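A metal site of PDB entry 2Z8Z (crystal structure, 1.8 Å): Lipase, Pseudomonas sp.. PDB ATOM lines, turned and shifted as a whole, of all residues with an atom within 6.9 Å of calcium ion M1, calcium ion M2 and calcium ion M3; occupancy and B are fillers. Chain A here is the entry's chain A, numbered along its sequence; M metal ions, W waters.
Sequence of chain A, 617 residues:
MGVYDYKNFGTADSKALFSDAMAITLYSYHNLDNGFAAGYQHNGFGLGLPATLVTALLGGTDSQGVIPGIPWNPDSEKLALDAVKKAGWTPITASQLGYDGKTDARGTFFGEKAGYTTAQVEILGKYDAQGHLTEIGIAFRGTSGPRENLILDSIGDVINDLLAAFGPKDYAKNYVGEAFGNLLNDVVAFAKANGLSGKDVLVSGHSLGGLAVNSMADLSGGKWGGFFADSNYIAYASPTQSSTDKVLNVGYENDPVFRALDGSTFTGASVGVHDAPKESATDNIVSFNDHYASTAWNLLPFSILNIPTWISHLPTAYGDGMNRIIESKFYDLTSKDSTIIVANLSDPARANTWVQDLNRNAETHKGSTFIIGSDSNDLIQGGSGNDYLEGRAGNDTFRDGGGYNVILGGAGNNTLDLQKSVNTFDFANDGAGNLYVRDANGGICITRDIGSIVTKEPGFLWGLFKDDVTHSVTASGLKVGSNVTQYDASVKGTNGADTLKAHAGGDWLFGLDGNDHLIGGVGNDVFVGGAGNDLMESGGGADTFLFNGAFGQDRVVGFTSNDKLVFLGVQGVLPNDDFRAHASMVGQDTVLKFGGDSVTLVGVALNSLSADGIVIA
Eight residues have an atom within 4 Å of calcium ion M1: Leu 512, Asp 513, Gly 514, Asp 516, Gly 529, Gly 530, Ala 531 and Asp 534. Along chain A the residues within 4 Å of calcium ion M1 span positions 512 to 534. The nearest printed residue that does not touch calcium ion M1 is Gly 511 (4.2 Å).
N of Gly 511 is in hydrogen-bond range of O of Val 528 (3.0 Å). The side-chain hydroxyl (OG1) of Thr 494 is in hydrogen-bond range of the backbone NH (N) of Gly 496. The side-chain amide nitrogen (ND2) of Asn 495 sits close to the backbone NH (N) of Asp 513 (3.1 Å). The backbone carbonyl oxygen (O) of Ser 598 lies within hydrogen-bond range of the backbone NH (N) of Asp 554, 2.9 Å away.
Calcium ion M2 is bound by O of Gly 511 (2.2 Å), O of Thr 494 (2.3 Å), O of Gly 496 (2.3 Å), O of Asp 513 (2.3 Å), OD2 of Asp 498 (2.4 Å), OD1 of Asp 516 (2.4 Å) and OD2 of Asp 516 (2.7 Å). Calcium ion M2 has seven donor atoms within binding distance.
Six residues have an atom within 4 Å of calcium ion M3: Gly 530, Ala 531, Gly 532, Asp 534, Phe 551 and Asp 554.
Calcium ion M3 is bound by the backbone carbonyl oxygen (O) of Phe 551 (2.2 Å). O of Gly 530 is bound to calcium ion M3 (2.2 Å). Calcium ion M3 is bound by O of Gly 532 (2.3 Å). The side-chain carboxylate (OD2) of Asp 534 is bound to calcium ion M3 (2.3 Å). OD1 of Asp 554 binds calcium ion M3 (2.4 Å). Calcium ion M3 is bound by water W1 (2.4 Å). Calcium ion M3 has six donor atoms within binding distance. Slightly farther from calcium ion M3 lies OD2 of Asp 554 (3.1 Å).
Water W1 lies within hydrogen-bond range of OD2 of Asp 554 (2.6 Å) and N of Gly 530 (3.4 Å).
Calcium ion M1 is bound by O of Leu 512 (2.3 Å), O of Gly 514 (2.3 Å), O of Ala 531 (2.3 Å), OD1 of Asp 534 (2.4 Å), O of Gly 529 (2.4 Å) and OD2 of Asp 516 (2.4 Å). Calcium ion M1 has six donor atoms within binding distance. Slightly farther from calcium ion M1 lies OD2 of Asp 534 (3.0 Å).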
ATOM      1  N   GLY A 493       8.346 -19.197 -32.289  1.00  0.00           N
ATOM      2  CA  GLY A 493       8.012 -20.602 -32.438  1.00  0.00           C
ATOM      3  C   GLY A 493       6.699 -20.890 -33.173  1.00  0.00           C
ATOM      4  O   GLY A 493       6.280 -20.147 -34.064  1.00  0.00           O
ATOM      5  N   THR A 494       6.054 -21.945 -32.763  1.00  0.00           N
ATOM      6  CA  THR A 494       4.796 -22.409 -33.293  1.00  0.00           C
ATOM      7  C   THR A 494       3.898 -22.798 -32.135  1.00  0.00           C
ATOM      8  O   THR A 494       4.339 -22.755 -30.996  1.00  0.00           O
ATOM      9  CB  THR A 494       5.031 -23.632 -34.182  1.00  0.00           C
ATOM     10  OG1 THR A 494       5.325 -24.786 -33.394  1.00  0.00           O
ATOM     11  CG2 THR A 494       6.105 -23.371 -35.222  1.00  0.00           C
ATOM     12  N   ASN A 495       2.661 -23.188 -32.422  1.00  0.00           N
ATOM     13  CA  ASN A 495       1.765 -23.666 -31.358  1.00  0.00           C
ATOM     14  C   ASN A 495       2.019 -25.127 -30.926  1.00  0.00           C
ATOM     15  O   ASN A 495       1.304 -25.647 -30.115  1.00  0.00           O
ATOM     16  CB  ASN A 495       0.305 -23.422 -31.740  1.00  0.00           C
ATOM     17  CG  ASN A 495      -0.078 -21.961 -31.606  1.00  0.00           C
ATOM     18  OD1 ASN A 495      -0.902 -21.465 -32.381  1.00  0.00           O
ATOM     19  ND2 ASN A 495       0.508 -21.269 -30.640  1.00  0.00           N
ATOM     20  N   GLY A 496       3.056 -25.773 -31.484  1.00  0.00           N
ATOM     21  CA  GLY A 496       3.553 -27.058 -30.992  1.00  0.00           C
ATOM     22  C   GLY A 496       4.832 -26.842 -30.158  1.00  0.00           C
ATOM     23  O   GLY A 496       5.204 -25.704 -29.881  1.00  0.00           O
ATOM     24  N   ALA A 497       5.462 -27.927 -29.783  1.00  0.00           N
ATOM     25  CA  ALA A 497       6.722 -27.916 -29.005  1.00  0.00           C
ATOM     26  C   ALA A 497       7.914 -27.519 -29.913  1.00  0.00           C
ATOM     27  O   ALA A 497       8.157 -28.171 -30.948  1.00  0.00           O
ATOM     28  CB  ALA A 497       6.938 -29.271 -28.444  1.00  0.00           C
ATOM     29  N   ASP A 498       8.575 -26.418 -29.567  1.00  0.00           N
ATOM     30  CA  ASP A 498       9.671 -25.888 -30.331  1.00  0.00           C
ATOM     31  C   ASP A 498      10.910 -25.788 -29.443  1.00  0.00           C
ATOM     32  O   ASP A 498      10.812 -25.569 -28.274  1.00  0.00           O
ATOM     33  CB  ASP A 498       9.407 -24.467 -30.764  1.00  0.00           C
ATOM     34  CG  ASP A 498       8.025 -24.251 -31.379  1.00  0.00           C
ATOM     35  OD1 ASP A 498       7.735 -24.821 -32.455  1.00  0.00           O
ATOM     36  OD2 ASP A 498       7.225 -23.460 -30.813  1.00  0.00           O
ATOM     37  N   LEU A 500      13.811 -23.007 -29.444  1.00  0.00           N
ATOM     38  CA  LEU A 500      14.224 -21.760 -30.012  1.00  0.00           C
ATOM     39  C   LEU A 500      15.533 -21.343 -29.336  1.00  0.00           C
ATOM     40  O   LEU A 500      15.654 -21.413 -28.132  1.00  0.00           O
ATOM     41  CB  LEU A 500      13.209 -20.663 -29.763  1.00  0.00           C
ATOM     42  CG  LEU A 500      11.742 -20.948 -30.075  1.00  0.00           C
ATOM     43  CD1 LEU A 500      10.976 -19.718 -29.724  1.00  0.00           C
ATOM     44  CD2 LEU A 500      11.548 -21.379 -31.581  1.00  0.00           C
ATOM     45  N   PHE A 510       9.656 -16.123 -28.388  1.00  0.00           N
ATOM     46  CA  PHE A 510       8.187 -16.339 -28.301  1.00  0.00           C
ATOM     47  C   PHE A 510       7.843 -17.823 -28.569  1.00  0.00           C
ATOM     48  O   PHE A 510       7.757 -18.276 -29.740  1.00  0.00           O
ATOM     49  CB  PHE A 510       7.501 -15.437 -29.335  1.00  0.00           C
ATOM     50  CG  PHE A 510       7.666 -13.967 -29.084  1.00  0.00           C
ATOM     51  CD1 PHE A 510       7.154 -13.364 -27.935  1.00  0.00           C
ATOM     52  CD2 PHE A 510       8.327 -13.134 -30.006  1.00  0.00           C
ATOM     53  CE1 PHE A 510       7.275 -12.019 -27.715  1.00  0.00           C
ATOM     54  CE2 PHE A 510       8.449 -11.752 -29.758  1.00  0.00           C
ATOM     55  CZ  PHE A 510       7.916 -11.204 -28.624  1.00  0.00           C
ATOM     56  N   GLY A 511       7.706 -18.611 -27.517  1.00  0.00           N
ATOM     57  CA  GLY A 511       7.397 -20.003 -27.656  1.00  0.00           C
ATOM     58  C   GLY A 511       5.993 -20.282 -28.179  1.00  0.00           C
ATOM     59  O   GLY A 511       5.759 -21.352 -28.806  1.00  0.00           O
ATOM     60  N   LEU A 512       5.070 -19.356 -27.884  1.00  0.00           N
ATOM     61  CA  LEU A 512       3.634 -19.570 -28.147  1.00  0.00           C
ATOM     62  C   LEU A 512       3.164 -20.898 -27.482  1.00  0.00           C
ATOM     63  O   LEU A 512       3.731 -21.341 -26.441  1.00  0.00           O
ATOM     64  CB  LEU A 512       3.396 -19.596 -29.651  1.00  0.00           C
ATOM     65  CG  LEU A 512       3.997 -18.453 -30.455  1.00  0.00           C
ATOM     66  CD1 LEU A 512       3.763 -18.663 -31.952  1.00  0.00           C
ATOM     67  CD2 LEU A 512       3.506 -17.102 -29.981  1.00  0.00           C
ATOM     68  N   ASP A 513       2.086 -21.508 -28.000  1.00  0.00           N
ATOM     69  CA  ASP A 513       1.552 -22.673 -27.350  1.00  0.00           C
ATOM     70  C   ASP A 513       2.493 -23.865 -27.411  1.00  0.00           C
ATOM     71  O   ASP A 513       3.442 -23.884 -28.208  1.00  0.00           O
ATOM     72  CB  ASP A 513       0.186 -23.084 -27.923  1.00  0.00           C
ATOM     73  CG  ASP A 513      -0.890 -21.985 -27.852  1.00  0.00           C
ATOM     74  OD1 ASP A 513      -0.690 -20.919 -27.214  1.00  0.00           O
ATOM     75  OD2 ASP A 513      -1.966 -22.247 -28.444  1.00  0.00           O
ATOM     76  N   GLY A 514       2.237 -24.857 -26.539  1.00  0.00           N
ATOM     77  CA  GLY A 514       2.966 -26.078 -26.464  1.00  0.00           C
ATOM     78  C   GLY A 514       4.147 -25.933 -25.492  1.00  0.00           C
ATOM     79  O   GLY A 514       4.461 -24.805 -25.049  1.00  0.00           O
ATOM     80  N   ASN A 515       4.779 -27.076 -25.192  1.00  0.00           N
ATOM     81  CA  ASN A 515       5.875 -27.167 -24.235  1.00  0.00           C
ATOM     82  C   ASN A 515       7.180 -26.884 -24.924  1.00  0.00           C
ATOM     83  O   ASN A 515       7.722 -27.736 -25.623  1.00  0.00           O
ATOM     84  CB  ASN A 515       5.876 -28.510 -23.534  1.00  0.00           C
ATOM     85  CG  ASN A 515       4.554 -28.839 -22.841  1.00  0.00           C
ATOM     86  OD1 ASN A 515       3.722 -27.971 -22.576  1.00  0.00           O
ATOM     87  ND2 ASN A 515       4.344 -30.093 -22.605  1.00  0.00           N
ATOM     88  N   ASP A 516       7.674 -25.671 -24.747  1.00  0.00           N
ATOM     89  CA  ASP A 516       8.839 -25.165 -25.484  1.00  0.00           C
ATOM     90  C   ASP A 516      10.136 -25.166 -24.665  1.00  0.00           C
ATOM     91  O   ASP A 516      10.117 -25.292 -23.456  1.00  0.00           O
ATOM     92  CB  ASP A 516       8.535 -23.793 -26.020  1.00  0.00           C
ATOM     93  CG  ASP A 516       7.275 -23.798 -26.902  1.00  0.00           C
ATOM     94  OD1 ASP A 516       7.229 -24.630 -27.870  1.00  0.00           O
ATOM     95  OD2 ASP A 516       6.385 -22.972 -26.625  1.00  0.00           O
ATOM     96  N   LEU A 518      13.372 -22.997 -24.531  1.00  0.00           N
ATOM     97  CA  LEU A 518      13.881 -21.711 -24.902  1.00  0.00           C
ATOM     98  C   LEU A 518      15.303 -21.493 -24.411  1.00  0.00           C
ATOM     99  O   LEU A 518      15.521 -21.407 -23.214  1.00  0.00           O
ATOM    100  CB  LEU A 518      12.987 -20.617 -24.365  1.00  0.00           C
ATOM    101  CG  LEU A 518      11.810 -20.234 -25.258  1.00  0.00           C
ATOM    102  CD1 LEU A 518      11.159 -21.292 -26.001  1.00  0.00           C
ATOM    103  CD2 LEU A 518      10.816 -19.309 -24.559  1.00  0.00           C
ATOM    104  N   VAL A 528       9.301 -15.302 -23.480  1.00  0.00           N
ATOM    105  CA  VAL A 528       7.844 -15.455 -23.358  1.00  0.00           C
ATOM    106  C   VAL A 528       7.438 -16.880 -23.730  1.00  0.00           C
ATOM    107  O   VAL A 528       7.139 -17.236 -24.915  1.00  0.00           O
ATOM    108  CB  VAL A 528       7.080 -14.438 -24.223  1.00  0.00           C
ATOM    109  CG1 VAL A 528       5.587 -14.472 -23.842  1.00  0.00           C
ATOM    110  CG2 VAL A 528       7.645 -13.015 -24.084  1.00  0.00           C
ATOM    111  N   GLY A 529       7.453 -17.753 -22.721  1.00  0.00           N
ATOM    112  CA  GLY A 529       7.151 -19.171 -22.951  1.00  0.00           C
ATOM    113  C   GLY A 529       5.776 -19.368 -23.567  1.00  0.00           C
ATOM    114  O   GLY A 529       5.548 -20.289 -24.345  1.00  0.00           O
ATOM    115  N   GLY A 530       4.851 -18.501 -23.198  1.00  0.00           N
ATOM    116  CA  GLY A 530       3.424 -18.675 -23.527  1.00  0.00           C
ATOM    117  C   GLY A 530       2.737 -19.821 -22.790  1.00  0.00           C
ATOM    118  O   GLY A 530       3.217 -20.367 -21.747  1.00  0.00           O
ATOM    119  N   ALA A 531       1.611 -20.229 -23.358  1.00  0.00           N
ATOM    120  CA  ALA A 531       0.919 -21.423 -22.892  1.00  0.00           C
ATOM    121  C   ALA A 531       1.800 -22.612 -22.996  1.00  0.00           C
ATOM    122  O   ALA A 531       2.779 -22.581 -23.768  1.00  0.00           O
ATOM    123  CB  ALA A 531      -0.346 -21.653 -23.723  1.00  0.00           C
ATOM    124  N   GLY A 532       1.492 -23.635 -22.221  1.00  0.00           N
ATOM    125  CA  GLY A 532       2.320 -24.790 -22.112  1.00  0.00           C
ATOM    126  C   GLY A 532       3.386 -24.682 -21.025  1.00  0.00           C
ATOM    127  O   GLY A 532       3.572 -23.641 -20.440  1.00  0.00           O
ATOM    128  N   ASN A 533       4.129 -25.754 -20.866  1.00  0.00           N
ATOM    129  CA  ASN A 533       5.118 -25.940 -19.769  1.00  0.00           C
ATOM    130  C   ASN A 533       6.448 -25.793 -20.469  1.00  0.00           C
ATOM    131  O   ASN A 533       6.904 -26.680 -21.186  1.00  0.00           O
ATOM    132  CB  ASN A 533       4.923 -27.304 -19.100  1.00  0.00           C
ATOM    133  CG  ASN A 533       3.469 -27.488 -18.590  1.00  0.00           C
ATOM    134  OD1 ASN A 533       2.755 -26.546 -18.343  1.00  0.00           O
ATOM    135  ND2 ASN A 533       3.073 -28.742 -18.409  1.00  0.00           N
ATOM    136  N   ASP A 534       7.007 -24.619 -20.313  1.00  0.00           N
ATOM    137  CA  ASP A 534       8.160 -24.225 -21.038  1.00  0.00           C
ATOM    138  C   ASP A 534       9.402 -24.316 -20.175  1.00  0.00           C
ATOM    139  O   ASP A 534       9.351 -23.906 -19.017  1.00  0.00           O
ATOM    140  CB  ASP A 534       7.977 -22.854 -21.548  1.00  0.00           C
ATOM    141  CG  ASP A 534       6.745 -22.723 -22.411  1.00  0.00           C
ATOM    142  OD1 ASP A 534       6.662 -23.369 -23.480  1.00  0.00           O
ATOM    143  OD2 ASP A 534       5.843 -22.009 -21.987  1.00  0.00           O
ATOM    144  N   MET A 536      13.082 -22.765 -19.838  1.00  0.00           N
ATOM    145  CA  MET A 536      13.673 -21.540 -20.281  1.00  0.00           C
ATOM    146  C   MET A 536      14.991 -21.283 -19.646  1.00  0.00           C
ATOM    147  O   MET A 536      15.081 -21.222 -18.428  1.00  0.00           O
ATOM    148  CB  MET A 536      12.715 -20.381 -20.087  1.00  0.00           C
ATOM    149  CG  MET A 536      11.348 -20.617 -20.720  1.00  0.00           C
ATOM    150  SD  MET A 536      10.256 -19.239 -20.550  1.00  0.00           S
ATOM    151  CE  MET A 536       9.551 -19.575 -18.989  1.00  0.00           C
ATOM    152  N   PHE A 547       5.393 -13.686 -17.893  1.00  0.00           N
ATOM    153  CA  PHE A 547       4.349 -14.664 -17.645  1.00  0.00           C
ATOM    154  C   PHE A 547       3.012 -13.931 -17.620  1.00  0.00           C
ATOM    155  O   PHE A 547       2.876 -12.974 -16.891  1.00  0.00           O
ATOM    156  CB  PHE A 547       4.574 -15.371 -16.325  1.00  0.00           C
ATOM    157  CG  PHE A 547       5.944 -15.968 -16.208  1.00  0.00           C
ATOM    158  CD1 PHE A 547       6.200 -17.227 -16.688  1.00  0.00           C
ATOM    159  CD2 PHE A 547       6.960 -15.266 -15.570  1.00  0.00           C
ATOM    160  CE1 PHE A 547       7.506 -17.774 -16.578  1.00  0.00           C
ATOM    161  CE2 PHE A 547       8.231 -15.791 -15.530  1.00  0.00           C
ATOM    162  CZ  PHE A 547       8.491 -17.042 -15.992  1.00  0.00           C
ATOM    163  N   ALA A 550      -2.856 -18.007 -18.494  1.00  0.00           N
ATOM    164  CA  ALA A 550      -2.740 -19.363 -17.929  1.00  0.00           C
ATOM    165  C   ALA A 550      -1.432 -19.917 -18.474  1.00  0.00           C
ATOM    166  O   ALA A 550      -1.387 -20.638 -19.494  1.00  0.00           O
ATOM    167  CB  ALA A 550      -3.901 -20.220 -18.320  1.00  0.00           C
ATOM    168  N   PHE A 551      -0.350 -19.523 -17.832  1.00  0.00           N
ATOM    169  CA  PHE A 551       0.986 -19.644 -18.452  1.00  0.00           C
ATOM    170  C   PHE A 551       1.642 -21.005 -18.271  1.00  0.00           C
ATOM    171  O   PHE A 551       2.698 -21.283 -18.826  1.00  0.00           O
ATOM    172  CB  PHE A 551       1.881 -18.513 -18.009  1.00  0.00           C
ATOM    173  CG  PHE A 551       2.185 -18.496 -16.529  1.00  0.00           C
ATOM    174  CD1 PHE A 551       3.170 -19.301 -16.012  1.00  0.00           C
ATOM    175  CD2 PHE A 551       1.515 -17.630 -15.691  1.00  0.00           C
ATOM    176  CE1 PHE A 551       3.462 -19.279 -14.588  1.00  0.00           C
ATOM    177  CE2 PHE A 551       1.798 -17.576 -14.348  1.00  0.00           C
ATOM    178  CZ  PHE A 551       2.757 -18.411 -13.777  1.00  0.00           C
ATOM    179  N   GLY A 552       0.985 -21.882 -17.511  1.00  0.00           N
ATOM    180  CA  GLY A 552       1.464 -23.252 -17.337  1.00  0.00           C
ATOM    181  C   GLY A 552       2.461 -23.470 -16.227  1.00  0.00           C
ATOM    182  O   GLY A 552       2.488 -22.694 -15.227  1.00  0.00           O
ATOM    183  N   GLN A 553       3.180 -24.595 -16.331  1.00  0.00           N
ATOM    184  CA  GLN A 553       4.151 -25.032 -15.304  1.00  0.00           C
ATOM    185  C   GLN A 553       5.511 -24.896 -15.995  1.00  0.00           C
ATOM    186  O   GLN A 553       5.932 -25.787 -16.769  1.00  0.00           O
ATOM    187  CB  GLN A 553       3.949 -26.454 -14.810  1.00  0.00           C
ATOM    188  CG  GLN A 553       2.498 -26.881 -14.707  1.00  0.00           C
ATOM    189  CD  GLN A 553       1.710 -25.988 -13.853  1.00  0.00           C
ATOM    190  OE1 GLN A 553       0.586 -25.608 -14.202  1.00  0.00           O
ATOM    191  NE2 GLN A 553       2.250 -25.642 -12.723  1.00  0.00           N
ATOM    192  N   ASP A 554       6.166 -23.783 -15.709  1.00  0.00           N
ATOM    193  CA  ASP A 554       7.422 -23.446 -16.378  1.00  0.00           C
ATOM    194  C   ASP A 554       8.613 -23.723 -15.459  1.00  0.00           C
ATOM    195  O   ASP A 554       8.449 -23.721 -14.251  1.00  0.00           O
ATOM    196  CB  ASP A 554       7.437 -21.978 -16.779  1.00  0.00           C
ATOM    197  CG  ASP A 554       6.380 -21.601 -17.812  1.00  0.00           C
ATOM    198  OD1 ASP A 554       5.980 -22.462 -18.701  1.00  0.00           O
ATOM    199  OD2 ASP A 554       5.999 -20.400 -17.750  1.00  0.00           O
ATOM    200  N   SER A 598       2.614 -22.087 -12.495  1.00  0.00           N
ATOM    201  CA  SER A 598       3.780 -22.078 -11.614  1.00  0.00           C
ATOM    202  C   SER A 598       5.050 -21.855 -12.414  1.00  0.00           C
ATOM    203  O   SER A 598       5.116 -22.155 -13.604  1.00  0.00           O
ATOM    204  CB  SER A 598       3.884 -23.370 -10.827  1.00  0.00           C
ATOM    205  OG  SER A 598       4.341 -24.459 -11.608  1.00  0.00           O
HETATM  206 CA    CA M   1       4.879 -22.525 -24.800  1.00  0.00          CA
HETATM  207 CA    CA M   2       5.553 -23.509 -29.156  1.00  0.00          CA
HETATM  208 CA    CA M   3       4.414 -21.463 -20.206  1.00  0.00          CA
HETATM  209  O   HOH W   1       5.348 -19.248 -19.965  1.00  0.00           O
